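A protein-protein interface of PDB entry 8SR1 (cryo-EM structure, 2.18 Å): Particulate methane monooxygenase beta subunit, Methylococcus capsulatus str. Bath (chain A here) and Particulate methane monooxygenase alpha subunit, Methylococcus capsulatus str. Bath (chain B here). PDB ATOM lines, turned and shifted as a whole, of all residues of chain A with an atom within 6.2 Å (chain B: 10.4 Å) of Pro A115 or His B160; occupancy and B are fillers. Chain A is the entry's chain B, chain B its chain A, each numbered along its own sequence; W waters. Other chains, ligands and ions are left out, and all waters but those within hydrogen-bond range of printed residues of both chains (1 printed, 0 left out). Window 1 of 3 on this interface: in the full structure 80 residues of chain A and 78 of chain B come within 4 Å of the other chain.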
ATOM      1  N   ASP A  43     -23.549  -9.778 -22.387  1.00  0.00           N
ATOM      2  CA  ASP A  43     -23.868  -9.128 -21.125  1.00  0.00           C
ATOM      3  C   ASP A  43     -24.815  -9.943 -20.256  1.00  0.00           C
ATOM      4  O   ASP A  43     -24.850  -9.733 -19.040  1.00  0.00           O
ATOM      5  CB  ASP A  43     -24.478  -7.748 -21.386  1.00  0.00           C
ATOM      6  CG  ASP A  43     -24.500  -6.879 -20.146  1.00  0.00           C
ATOM      7  OD1 ASP A  43     -23.415  -6.592 -19.601  1.00  0.00           O
ATOM      8  OD2 ASP A  43     -25.606  -6.493 -19.710  1.00  0.00           O
ATOM      9  N   PHE A  44     -25.571 -10.871 -20.842  1.00  0.00           N
ATOM     10  CA  PHE A  44     -26.541 -11.656 -20.090  1.00  0.00           C
ATOM     11  C   PHE A  44     -25.902 -12.753 -19.249  1.00  0.00           C
ATOM     12  O   PHE A  44     -26.401 -13.060 -18.162  1.00  0.00           O
ATOM     13  CB  PHE A  44     -27.562 -12.288 -21.041  1.00  0.00           C
ATOM     14  CG  PHE A  44     -28.550 -11.314 -21.610  1.00  0.00           C
ATOM     15  CD1 PHE A  44     -28.689 -10.048 -21.070  1.00  0.00           C
ATOM     16  CD2 PHE A  44     -29.335 -11.665 -22.694  1.00  0.00           C
ATOM     17  CE1 PHE A  44     -29.595  -9.153 -21.598  1.00  0.00           C
ATOM     18  CE2 PHE A  44     -30.243 -10.773 -23.227  1.00  0.00           C
ATOM     19  CZ  PHE A  44     -30.372  -9.515 -22.678  1.00  0.00           C
ATOM     20  N   LYS A  49     -19.220 -14.218 -20.837  1.00  0.00           N
ATOM     21  CA  LYS A  49     -18.180 -13.213 -20.586  1.00  0.00           C
ATOM     22  C   LYS A  49     -16.799 -13.833 -20.807  1.00  0.00           C
ATOM     23  O   LYS A  49     -16.099 -14.229 -19.871  1.00  0.00           O
ATOM     24  CB  LYS A  49     -18.298 -12.645 -19.177  1.00  0.00           C
ATOM     25  CG  LYS A  49     -19.708 -12.322 -18.743  1.00  0.00           C
ATOM     26  CD  LYS A  49     -19.989 -10.837 -18.807  1.00  0.00           C
ATOM     27  CE  LYS A  49     -21.217 -10.476 -18.000  1.00  0.00           C
ATOM     28  NZ  LYS A  49     -22.440 -11.080 -18.586  1.00  0.00           N
ATOM     29  N   LEU A  91     -26.524   0.901 -17.168  1.00  0.00           N
ATOM     30  CA  LEU A  91     -26.343   0.003 -16.030  1.00  0.00           C
ATOM     31  C   LEU A  91     -27.606  -0.081 -15.187  1.00  0.00           C
ATOM     32  O   LEU A  91     -27.963  -1.160 -14.707  1.00  0.00           O
ATOM     33  CB  LEU A  91     -25.161   0.464 -15.182  1.00  0.00           C
ATOM     34  CG  LEU A  91     -23.780   0.054 -15.694  1.00  0.00           C
ATOM     35  CD1 LEU A  91     -22.698   0.870 -15.019  1.00  0.00           C
ATOM     36  CD2 LEU A  91     -23.550  -1.428 -15.469  1.00  0.00           C
ATOM     37  N   GLU A  94     -30.174  -2.186 -17.135  1.00  0.00           N
ATOM     38  CA  GLU A  94     -29.733  -3.572 -17.162  1.00  0.00           C
ATOM     39  C   GLU A  94     -29.920  -4.233 -15.805  1.00  0.00           C
ATOM     40  O   GLU A  94     -30.429  -5.352 -15.719  1.00  0.00           O
ATOM     41  CB  GLU A  94     -28.272  -3.646 -17.606  1.00  0.00           C
ATOM     42  CG  GLU A  94     -28.085  -3.575 -19.110  1.00  0.00           C
ATOM     43  CD  GLU A  94     -26.629  -3.465 -19.516  1.00  0.00           C
ATOM     44  OE1 GLU A  94     -25.834  -2.906 -18.733  1.00  0.00           O
ATOM     45  OE2 GLU A  94     -26.283  -3.929 -20.621  1.00  0.00           O
ATOM     46  N   TRP A  95     -29.527  -3.550 -14.727  1.00  0.00           N
ATOM     47  CA  TRP A  95     -29.656  -4.125 -13.393  1.00  0.00           C
ATOM     48  C   TRP A  95     -31.110  -4.287 -12.987  1.00  0.00           C
ATOM     49  O   TRP A  95     -31.469  -5.292 -12.361  1.00  0.00           O
ATOM     50  CB  TRP A  95     -28.915  -3.267 -12.369  1.00  0.00           C
ATOM     51  CG  TRP A  95     -27.535  -3.759 -12.077  1.00  0.00           C
ATOM     52  CD1 TRP A  95     -26.363  -3.131 -12.374  1.00  0.00           C
ATOM     53  CD2 TRP A  95     -27.182  -4.988 -11.436  1.00  0.00           C
ATOM     54  NE1 TRP A  95     -25.300  -3.892 -11.957  1.00  0.00           N
ATOM     55  CE2 TRP A  95     -25.775  -5.038 -11.374  1.00  0.00           C
ATOM     56  CE3 TRP A  95     -27.916  -6.053 -10.906  1.00  0.00           C
ATOM     57  CZ2 TRP A  95     -25.091  -6.107 -10.807  1.00  0.00           C
ATOM     58  CZ3 TRP A  95     -27.234  -7.112 -10.342  1.00  0.00           C
ATOM     59  CH2 TRP A  95     -25.836  -7.132 -10.297  1.00  0.00           C
ATOM     60  N   ARG A  98     -32.245  -7.342 -14.817  1.00  0.00           N
ATOM     61  CA  ARG A  98     -31.626  -8.542 -14.262  1.00  0.00           C
ATOM     62  C   ARG A  98     -32.297  -8.945 -12.959  1.00  0.00           C
ATOM     63  O   ARG A  98     -32.606 -10.125 -12.750  1.00  0.00           O
ATOM     64  CB  ARG A  98     -30.132  -8.319 -14.011  1.00  0.00           C
ATOM     65  CG  ARG A  98     -29.266  -8.051 -15.227  1.00  0.00           C
ATOM     66  CD  ARG A  98     -29.691  -8.826 -16.446  1.00  0.00           C
ATOM     67  NE  ARG A  98     -29.388  -8.084 -17.662  1.00  0.00           N
ATOM     68  CZ  ARG A  98     -28.193  -8.042 -18.236  1.00  0.00           C
ATOM     69  NH1 ARG A  98     -27.160  -8.700 -17.733  1.00  0.00           N
ATOM     70  NH2 ARG A  98     -28.028  -7.319 -19.339  1.00  0.00           N
ATOM     71  N   ILE A 110     -28.295 -14.048  -9.703  1.00  0.00           N
ATOM     72  CA  ILE A 110     -27.673 -12.775 -10.049  1.00  0.00           C
ATOM     73  C   ILE A 110     -26.205 -12.973 -10.400  1.00  0.00           C
ATOM     74  O   ILE A 110     -25.680 -12.336 -11.325  1.00  0.00           O
ATOM     75  CB  ILE A 110     -27.857 -11.765  -8.901  1.00  0.00           C
ATOM     76  CG1 ILE A 110     -29.341 -11.451  -8.711  1.00  0.00           C
ATOM     77  CG2 ILE A 110     -27.056 -10.498  -9.157  1.00  0.00           C
ATOM     78  CD1 ILE A 110     -29.882 -10.418  -9.670  1.00  0.00           C
ATOM     79  N   VAL A 113     -26.376 -13.815 -14.010  1.00  0.00           N
ATOM     80  CA  VAL A 113     -26.927 -12.888 -14.996  1.00  0.00           C
ATOM     81  C   VAL A 113     -26.510 -11.440 -14.730  1.00  0.00           C
ATOM     82  O   VAL A 113     -27.170 -10.517 -15.196  1.00  0.00           O
ATOM     83  CB  VAL A 113     -28.456 -13.014 -15.084  1.00  0.00           C
ATOM     84  CG1 VAL A 113     -28.840 -14.391 -15.590  1.00  0.00           C
ATOM     85  CG2 VAL A 113     -29.096 -12.731 -13.735  1.00  0.00           C
ATOM     86  N   PHE A 114     -25.420 -11.220 -13.999  1.00  0.00           N
ATOM     87  CA  PHE A 114     -24.976  -9.858 -13.736  1.00  0.00           C
ATOM     88  C   PHE A 114     -24.492  -9.184 -15.024  1.00  0.00           C
ATOM     89  O   PHE A 114     -23.972  -9.845 -15.923  1.00  0.00           O
ATOM     90  CB  PHE A 114     -23.854  -9.854 -12.704  1.00  0.00           C
ATOM     91  CG  PHE A 114     -22.628 -10.595 -13.142  1.00  0.00           C
ATOM     92  CD1 PHE A 114     -22.503 -11.952 -12.908  1.00  0.00           C
ATOM     93  CD2 PHE A 114     -21.595  -9.935 -13.786  1.00  0.00           C
ATOM     94  CE1 PHE A 114     -21.379 -12.636 -13.313  1.00  0.00           C
ATOM     95  CE2 PHE A 114     -20.468 -10.616 -14.193  1.00  0.00           C
ATOM     96  CZ  PHE A 114     -20.360 -11.968 -13.954  1.00  0.00           C
ATOM     97  N   PRO A 115     -24.650  -7.870 -15.130  1.00  0.00           N
ATOM     98  CA  PRO A 115     -24.126  -7.134 -16.285  1.00  0.00           C
ATOM     99  C   PRO A 115     -22.653  -6.783 -16.092  1.00  0.00           C
ATOM    100  O   PRO A 115     -22.072  -6.963 -15.024  1.00  0.00           O
ATOM    101  CB  PRO A 115     -24.998  -5.880 -16.319  1.00  0.00           C
ATOM    102  CG  PRO A 115     -25.367  -5.660 -14.898  1.00  0.00           C
ATOM    103  CD  PRO A 115     -25.480  -7.017 -14.262  1.00  0.00           C
ATOM    104  N   ALA A 116     -22.050  -6.271 -17.163  1.00  0.00           N
ATOM    105  CA  ALA A 116     -20.665  -5.825 -17.146  1.00  0.00           C
ATOM    106  C   ALA A 116     -20.555  -4.417 -16.574  1.00  0.00           C
ATOM    107  O   ALA A 116     -21.528  -3.661 -16.537  1.00  0.00           O
ATOM    108  CB  ALA A 116     -20.069  -5.861 -18.553  1.00  0.00           C
ATOM    109  N   SER A 117     -19.350  -4.070 -16.124  1.00  0.00           N
ATOM    110  CA  SER A 117     -19.065  -2.750 -15.577  1.00  0.00           C
ATOM    111  C   SER A 117     -18.465  -1.856 -16.659  1.00  0.00           C
ATOM    112  O   SER A 117     -17.611  -2.298 -17.432  1.00  0.00           O
ATOM    113  CB  SER A 117     -18.110  -2.861 -14.387  1.00  0.00           C
ATOM    114  OG  SER A 117     -17.862  -1.593 -13.808  1.00  0.00           O
ATOM    115  N   LEU A 118     -18.920  -0.597 -16.711  1.00  0.00           N
ATOM    116  CA  LEU A 118     -18.513   0.340 -17.756  1.00  0.00           C
ATOM    117  C   LEU A 118     -18.158   1.723 -17.215  1.00  0.00           C
ATOM    118  O   LEU A 118     -17.689   2.582 -17.983  1.00  0.00           O
ATOM    119  CB  LEU A 118     -19.620   0.472 -18.804  1.00  0.00           C
ATOM    120  CG  LEU A 118     -20.214  -0.843 -19.302  1.00  0.00           C
ATOM    121  CD1 LEU A 118     -21.695  -0.685 -19.606  1.00  0.00           C
ATOM    122  CD2 LEU A 118     -19.441  -1.357 -20.501  1.00  0.00           C
ATOM    123  N   VAL A 119     -18.383   1.963 -15.921  1.00  0.00           N
ATOM    124  CA  VAL A 119     -18.120   3.284 -15.350  1.00  0.00           C
ATOM    125  C   VAL A 119     -16.669   3.721 -15.519  1.00  0.00           C
ATOM    126  O   VAL A 119     -16.435   4.911 -15.777  1.00  0.00           O
ATOM    127  CB  VAL A 119     -18.583   3.328 -13.885  1.00  0.00           C
ATOM    128  CG1 VAL A 119     -18.088   4.597 -13.209  1.00  0.00           C
ATOM    129  CG2 VAL A 119     -20.095   3.249 -13.812  1.00  0.00           C
ATOM    130  N   ASN A 154     -13.620  -5.197 -15.321  1.00  0.00           N
ATOM    131  CA  ASN A 154     -14.526  -6.283 -14.980  1.00  0.00           C
ATOM    132  C   ASN A 154     -13.821  -7.494 -14.388  1.00  0.00           C
ATOM    133  O   ASN A 154     -14.500  -8.411 -13.913  1.00  0.00           O
ATOM    134  CB  ASN A 154     -15.318  -6.722 -16.215  1.00  0.00           C
ATOM    135  CG  ASN A 154     -16.378  -5.719 -16.611  1.00  0.00           C
ATOM    136  OD1 ASN A 154     -17.485  -5.727 -16.075  1.00  0.00           O
ATOM    137  ND2 ASN A 154     -16.047  -4.851 -17.557  1.00  0.00           N
ATOM    138  N   ILE A 157     -14.761  -8.778 -10.861  1.00  0.00           N
ATOM    139  CA  ILE A 157     -16.071  -9.413 -10.759  1.00  0.00           C
ATOM    140  C   ILE A 157     -16.027 -10.845 -11.280  1.00  0.00           C
ATOM    141  O   ILE A 157     -16.543 -11.767 -10.642  1.00  0.00           O
ATOM    142  CB  ILE A 157     -17.128  -8.577 -11.501  1.00  0.00           C
ATOM    143  CG1 ILE A 157     -17.221  -7.174 -10.895  1.00  0.00           C
ATOM    144  CG2 ILE A 157     -18.480  -9.262 -11.463  1.00  0.00           C
ATOM    145  CD1 ILE A 157     -17.671  -6.119 -11.876  1.00  0.00           C
ATOM    146  N   ASN B 152     -19.958 -15.499  -5.288  1.00  0.00           N
ATOM    147  CA  ASN B 152     -19.521 -14.277  -5.963  1.00  0.00           C
ATOM    148  C   ASN B 152     -20.611 -13.212  -6.041  1.00  0.00           C
ATOM    149  O   ASN B 152     -20.357 -12.126  -6.586  1.00  0.00           O
ATOM    150  CB  ASN B 152     -18.987 -14.558  -7.377  1.00  0.00           C
ATOM    151  CG  ASN B 152     -18.112 -13.443  -7.902  1.00  0.00           C
ATOM    152  OD1 ASN B 152     -17.243 -12.937  -7.196  1.00  0.00           O
ATOM    153  ND2 ASN B 152     -18.336 -13.053  -9.149  1.00  0.00           N
ATOM    154  N   GLU B 153     -21.805 -13.472  -5.510  1.00  0.00           N
ATOM    155  CA  GLU B 153     -22.888 -12.495  -5.583  1.00  0.00           C
ATOM    156  C   GLU B 153     -22.535 -11.224  -4.817  1.00  0.00           C
ATOM    157  O   GLU B 153     -22.762 -10.106  -5.302  1.00  0.00           O
ATOM    158  CB  GLU B 153     -24.177 -13.108  -5.040  1.00  0.00           C
ATOM    159  CG  GLU B 153     -25.441 -12.375  -5.433  1.00  0.00           C
ATOM    160  CD  GLU B 153     -26.664 -12.905  -4.713  1.00  0.00           C
ATOM    161  OE1 GLU B 153     -26.922 -14.125  -4.795  1.00  0.00           O
ATOM    162  OE2 GLU B 153     -27.368 -12.107  -4.061  1.00  0.00           O
ATOM    163  N   GLY B 154     -21.986 -11.377  -3.612  1.00  0.00           N
ATOM    164  CA  GLY B 154     -21.601 -10.214  -2.831  1.00  0.00           C
ATOM    165  C   GLY B 154     -20.531  -9.388  -3.511  1.00  0.00           C
ATOM    166  O   GLY B 154     -20.597  -8.159  -3.536  1.00  0.00           O
ATOM    167  N   ASN B 155     -19.522 -10.056  -4.077  1.00  0.00           N
ATOM    168  CA  ASN B 155     -18.455  -9.350  -4.775  1.00  0.00           C
ATOM    169  C   ASN B 155     -18.990  -8.600  -5.989  1.00  0.00           C
ATOM    170  O   ASN B 155     -18.622  -7.442  -6.232  1.00  0.00           O
ATOM    171  CB  ASN B 155     -17.367 -10.341  -5.184  1.00  0.00           C
ATOM    172  CG  ASN B 155     -16.248  -9.693  -5.969  1.00  0.00           C
ATOM    173  OD1 ASN B 155     -15.535  -8.836  -5.457  1.00  0.00           O
ATOM    174  ND2 ASN B 155     -16.084 -10.114  -7.218  1.00  0.00           N
ATOM    175  N   THR B 156     -19.867  -9.246  -6.763  1.00  0.00           N
ATOM    176  CA  THR B 156     -20.464  -8.591  -7.922  1.00  0.00           C
ATOM    177  C   THR B 156     -21.262  -7.360  -7.509  1.00  0.00           C
ATOM    178  O   THR B 156     -21.096  -6.278  -8.093  1.00  0.00           O
ATOM    179  CB  THR B 156     -21.362  -9.571  -8.676  1.00  0.00           C
ATOM    180  OG1 THR B 156     -20.589 -10.695  -9.114  1.00  0.00           O
ATOM    181  CG2 THR B 156     -21.989  -8.894  -9.877  1.00  0.00           C
ATOM    182  N   TYR B 157     -22.124  -7.510  -6.500  1.00  0.00           N
ATOM    183  CA  TYR B 157     -22.907  -6.383  -6.012  1.00  0.00           C
ATOM    184  C   TYR B 157     -22.005  -5.254  -5.537  1.00  0.00           C
ATOM    185  O   TYR B 157     -22.239  -4.083  -5.852  1.00  0.00           O
ATOM    186  CB  TYR B 157     -23.830  -6.833  -4.880  1.00  0.00           C
ATOM    187  CG  TYR B 157     -25.140  -7.420  -5.339  1.00  0.00           C
ATOM    188  CD1 TYR B 157     -25.785  -6.936  -6.468  1.00  0.00           C
ATOM    189  CD2 TYR B 157     -25.742  -8.454  -4.635  1.00  0.00           C
ATOM    190  CE1 TYR B 157     -26.984  -7.466  -6.887  1.00  0.00           C
ATOM    191  CE2 TYR B 157     -26.940  -8.990  -5.047  1.00  0.00           C
ATOM    192  CZ  TYR B 157     -27.559  -8.494  -6.171  1.00  0.00           C
ATOM    193  OH  TYR B 157     -28.758  -9.028  -6.581  1.00  0.00           O
ATOM    194  N   PHE B 158     -20.957  -5.593  -4.784  1.00  0.00           N
ATOM    195  CA  PHE B 158     -20.065  -4.577  -4.238  1.00  0.00           C
ATOM    196  C   PHE B 158     -19.394  -3.784  -5.347  1.00  0.00           C
ATOM    197  O   PHE B 158     -19.379  -2.550  -5.324  1.00  0.00           O
ATOM    198  CB  PHE B 158     -19.014  -5.228  -3.339  1.00  0.00           C
ATOM    199  CG  PHE B 158     -17.847  -4.332  -3.036  1.00  0.00           C
ATOM    200  CD1 PHE B 158     -17.931  -3.383  -2.031  1.00  0.00           C
ATOM    201  CD2 PHE B 158     -16.669  -4.434  -3.759  1.00  0.00           C
ATOM    202  CE1 PHE B 158     -16.865  -2.554  -1.752  1.00  0.00           C
ATOM    203  CE2 PHE B 158     -15.600  -3.605  -3.485  1.00  0.00           C
ATOM    204  CZ  PHE B 158     -15.697  -2.665  -2.478  1.00  0.00           C
ATOM    205  N   TRP B 159     -18.815  -4.479  -6.327  1.00  0.00           N
ATOM    206  CA  TRP B 159     -18.087  -3.769  -7.373  1.00  0.00           C
ATOM    207  C   TRP B 159     -19.022  -2.928  -8.232  1.00  0.00           C
ATOM    208  O   TRP B 159     -18.698  -1.780  -8.577  1.00  0.00           O
ATOM    209  CB  TRP B 159     -17.297  -4.758  -8.228  1.00  0.00           C
ATOM    210  CG  TRP B 159     -15.999  -5.128  -7.597  1.00  0.00           C
ATOM    211  CD1 TRP B 159     -15.616  -6.365  -7.174  1.00  0.00           C
ATOM    212  CD2 TRP B 159     -14.917  -4.244  -7.283  1.00  0.00           C
ATOM    213  NE1 TRP B 159     -14.359  -6.310  -6.629  1.00  0.00           N
ATOM    214  CE2 TRP B 159     -13.906  -5.019  -6.683  1.00  0.00           C
ATOM    215  CE3 TRP B 159     -14.701  -2.874  -7.459  1.00  0.00           C
ATOM    216  CZ2 TRP B 159     -12.701  -4.470  -6.259  1.00  0.00           C
ATOM    217  CZ3 TRP B 159     -13.505  -2.332  -7.037  1.00  0.00           C
ATOM    218  CH2 TRP B 159     -12.521  -3.127  -6.442  1.00  0.00           C
ATOM    219  N   HIS B 160     -20.194  -3.470  -8.576  1.00  0.00           N
ATOM    220  CA  HIS B 160     -21.132  -2.694  -9.381  1.00  0.00           C
ATOM    221  C   HIS B 160     -21.617  -1.463  -8.626  1.00  0.00           C
ATOM    222  O   HIS B 160     -21.683  -0.368  -9.196  1.00  0.00           O
ATOM    223  CB  HIS B 160     -22.303  -3.570  -9.816  1.00  0.00           C
ATOM    224  CG  HIS B 160     -22.090  -4.234 -11.140  1.00  0.00           C
ATOM    225  ND1 HIS B 160     -22.279  -3.579 -12.338  1.00  0.00           N
ATOM    226  CD2 HIS B 160     -21.686  -5.486 -11.455  1.00  0.00           C
ATOM    227  CE1 HIS B 160     -22.008  -4.404 -13.333  1.00  0.00           C
ATOM    228  NE2 HIS B 160     -21.645  -5.567 -12.825  1.00  0.00           N
ATOM    229  N   ALA B 161     -21.940  -1.616  -7.337  1.00  0.00           N
ATOM    230  CA  ALA B 161     -22.364  -0.476  -6.537  1.00  0.00           C
ATOM    231  C   ALA B 161     -21.249   0.552  -6.405  1.00  0.00           C
ATOM    232  O   ALA B 161     -21.507   1.757  -6.449  1.00  0.00           O
ATOM    233  CB  ALA B 161     -22.829  -0.945  -5.159  1.00  0.00           C
ATOM    234  N   PHE B 162     -20.005   0.098  -6.244  1.00  0.00           N
ATOM    235  CA  PHE B 162     -18.880   1.017  -6.120  1.00  0.00           C
ATOM    236  C   PHE B 162     -18.716   1.861  -7.377  1.00  0.00           C
ATOM    237  O   PHE B 162     -18.579   3.090  -7.305  1.00  0.00           O
ATOM    238  CB  PHE B 162     -17.604   0.224  -5.821  1.00  0.00           C
ATOM    239  CG  PHE B 162     -16.346   1.042  -5.867  1.00  0.00           C
ATOM    240  CD1 PHE B 162     -15.893   1.701  -4.736  1.00  0.00           C
ATOM    241  CD2 PHE B 162     -15.600   1.132  -7.034  1.00  0.00           C
ATOM    242  CE1 PHE B 162     -14.732   2.448  -4.772  1.00  0.00           C
ATOM    243  CE2 PHE B 162     -14.440   1.878  -7.074  1.00  0.00           C
ATOM    244  CZ  PHE B 162     -14.004   2.535  -5.942  1.00  0.00           C
ATOM    245  N   TRP B 163     -18.734   1.219  -8.546  1.00  0.00           N
ATOM    246  CA  TRP B 163     -18.537   1.983  -9.775  1.00  0.00           C
ATOM    247  C   TRP B 163     -19.736   2.876 -10.074  1.00  0.00           C
ATOM    248  O   TRP B 163     -19.574   4.015 -10.539  1.00  0.00           O
ATOM    249  CB  TRP B 163     -18.237   1.037 -10.936  1.00  0.00           C
ATOM    250  CG  TRP B 163     -16.828   0.538 -10.893  1.00  0.00           C
ATOM    251  CD1 TRP B 163     -16.420  -0.756 -10.769  1.00  0.00           C
ATOM    252  CD2 TRP B 163     -15.635   1.332 -10.935  1.00  0.00           C
ATOM    253  NE1 TRP B 163     -15.049  -0.820 -10.748  1.00  0.00           N
ATOM    254  CE2 TRP B 163     -14.543   0.448 -10.848  1.00  0.00           C
ATOM    255  CE3 TRP B 163     -15.385   2.705 -11.049  1.00  0.00           C
ATOM    256  CZ2 TRP B 163     -13.223   0.889 -10.870  1.00  0.00           C
ATOM    257  CZ3 TRP B 163     -14.075   3.140 -11.070  1.00  0.00           C
ATOM    258  CH2 TRP B 163     -13.012   2.235 -10.981  1.00  0.00           C
ATOM    259  N   PHE B 164     -20.949   2.393  -9.790  1.00  0.00           N
ATOM    260  CA  PHE B 164     -22.128   3.236  -9.946  1.00  0.00           C
ATOM    261  C   PHE B 164     -22.049   4.453  -9.033  1.00  0.00           C
ATOM    262  O   PHE B 164     -22.419   5.562  -9.431  1.00  0.00           O
ATOM    263  CB  PHE B 164     -23.390   2.425  -9.657  1.00  0.00           C
ATOM    264  CG  PHE B 164     -24.618   2.963 -10.322  1.00  0.00           C
ATOM    265  CD1 PHE B 164     -25.382   3.943  -9.711  1.00  0.00           C
ATOM    266  CD2 PHE B 164     -25.019   2.487 -11.560  1.00  0.00           C
ATOM    267  CE1 PHE B 164     -26.517   4.440 -10.321  1.00  0.00           C
ATOM    268  CE2 PHE B 164     -26.151   2.981 -12.175  1.00  0.00           C
ATOM    269  CZ  PHE B 164     -26.900   3.960 -11.554  1.00  0.00           C
ATOM    270  N   ALA B 165     -21.566   4.261  -7.803  1.00  0.00           N
ATOM    271  CA  ALA B 165     -21.408   5.374  -6.874  1.00  0.00           C
ATOM    272  C   ALA B 165     -20.375   6.369  -7.378  1.00  0.00           C
ATOM    273  O   ALA B 165     -20.550   7.579  -7.226  1.00  0.00           O
ATOM    274  CB  ALA B 165     -21.025   4.855  -5.491  1.00  0.00           C
ATOM    275  N   ILE B 166     -19.282   5.879  -7.967  1.00  0.00           N
ATOM    276  CA  ILE B 166     -18.280   6.786  -8.530  1.00  0.00           C
ATOM    277  C   ILE B 166     -18.892   7.642  -9.633  1.00  0.00           C
ATOM    278  O   ILE B 166     -18.716   8.871  -9.669  1.00  0.00           O
ATOM    279  CB  ILE B 166     -17.063   5.988  -9.040  1.00  0.00           C
ATOM    280  CG1 ILE B 166     -16.204   5.506  -7.870  1.00  0.00           C
ATOM    281  CG2 ILE B 166     -16.235   6.830  -9.996  1.00  0.00           C
ATOM    282  CD1 ILE B 166     -15.690   6.621  -6.990  1.00  0.00           C
ATOM    283  N   GLY B 167     -19.633   7.008 -10.548  1.00  0.00           N
ATOM    284  CA  GLY B 167     -20.272   7.767 -11.617  1.00  0.00           C
ATOM    285  C   GLY B 167     -21.292   8.765 -11.097  1.00  0.00           C
ATOM    286  O   GLY B 167     -21.357   9.908 -11.566  1.00  0.00           O
ATOM    287  N   VAL B 168     -22.102   8.346 -10.122  1.00  0.00           N
ATOM    288  CA  VAL B 168     -23.095   9.237  -9.533  1.00  0.00           C
ATOM    289  C   VAL B 168     -22.419  10.401  -8.826  1.00  0.00           C
ATOM    290  O   VAL B 168     -22.915  11.530  -8.851  1.00  0.00           O
ATOM    291  CB  VAL B 168     -24.021   8.446  -8.584  1.00  0.00           C
ATOM    292  CG1 VAL B 168     -24.814   9.384  -7.691  1.00  0.00           C
ATOM    293  CG2 VAL B 168     -24.960   7.559  -9.388  1.00  0.00           C
HETATM  294  O   HOH W   1     -26.596 -15.319  -7.017  1.00  0.00           O
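The side-chain amide nitrogen of Asn B152 lies within hydrogen-bond range of the backbone carbonyl oxygen of Ile A157 (2.7 Å). A ring nitrogen (ND1) of His B160 is in hydrogen-bond range of the indole nitrogen of Trp A95 (3.1 Å). The backbone carbonyl oxygen (O) of Pro A115 is in hydrogen-bond range of a ring nitrogen (NE2) of His B160 (2.6 Å).
OD1 of Asn B152 is in hydrogen-bond range of ND2 of Asn B155, at 3.1 Å. The backbone carbonyl oxygen (O) of Asn B152 lies within hydrogen-bond range of the side-chain hydroxyl (OG1) of Thr B156 (2.9 Å). OD1 of Asn B155 sits close to NE1 of Trp B159 (3.0 Å). The backbone NH (N) of Ala A116 is in hydrogen-bond range of the side-chain carboxylate (OD1) of Asp A43. The side-chain amino group of Lys A49 is in hydrogen-bond range of the backbone carbonyl oxygen of Phe A114, 3.3 Å away. The side-chain amide oxygen of Asn A154 sits at hydrogen-bond distance from the backbone NH of Ser A117.
CD2 of Leu A91 touches CE1 of His B160 (3.97 Å). Trp A95 touches Tyr B157. Ile A110 touches Tyr B157 (CG1 to OH, 3.3 Å). Thr B156 touches Phe A114 (CG2 to CB, 3.5 Å). N of Ser A117 touches CE1 of His B160, at 3.9 Å. OG of Ser A117 touches CD1 of Trp B163, 3.5 Å away. Val A119 touches Gly B167. Asn B155 touches Ile A157 (ND2 to CA, 3.6 Å). OG1 of Thr B156 touches CG2 of Ile A157, at 3.5 Å. CG1 of Ile A157 touches CB of Trp B159, 3.6 Å away.
No residue of chain B comes within 4 Å of Glu A94. Phe A114 touches one residue of chain B. Of chain B, only His B160 comes within 4 Å of Pro A115. Printed residues of chain B within 4 Å of Ala A116: His B160. Of the printed residues of chain A, Asn B152 touches Ile A157 (2.7 Å). Of chain A, only Leu A91, Trp A95, Pro A115, Ala A116 and Ser A117 come within 4 Å of His B160. Printed residues of chain A within 4 Å of Gly B167: Val A119 (3.9 Å).
Of the 17 printed residues of chain A, 9 touch a printed residue of chain B. Hydrophobic or aromatic side chains of chain A within 4 Å of the printed part of chain B: Leu A91, Trp A95, Ile A110, Phe A114, Pro A115, Val A119 and Ile A157. Among the printed residues, no Asp or Glu carboxylate lies within 4 Å of a Lys or Arg side-chain nitrogen of the other chain.
Water W1 lies within hydrogen-bond range of the side-chain carboxylate (OE1) of Glu B153 (2.5 Å) and the backbone NH (N) of Ile A110 (3.4 Å).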
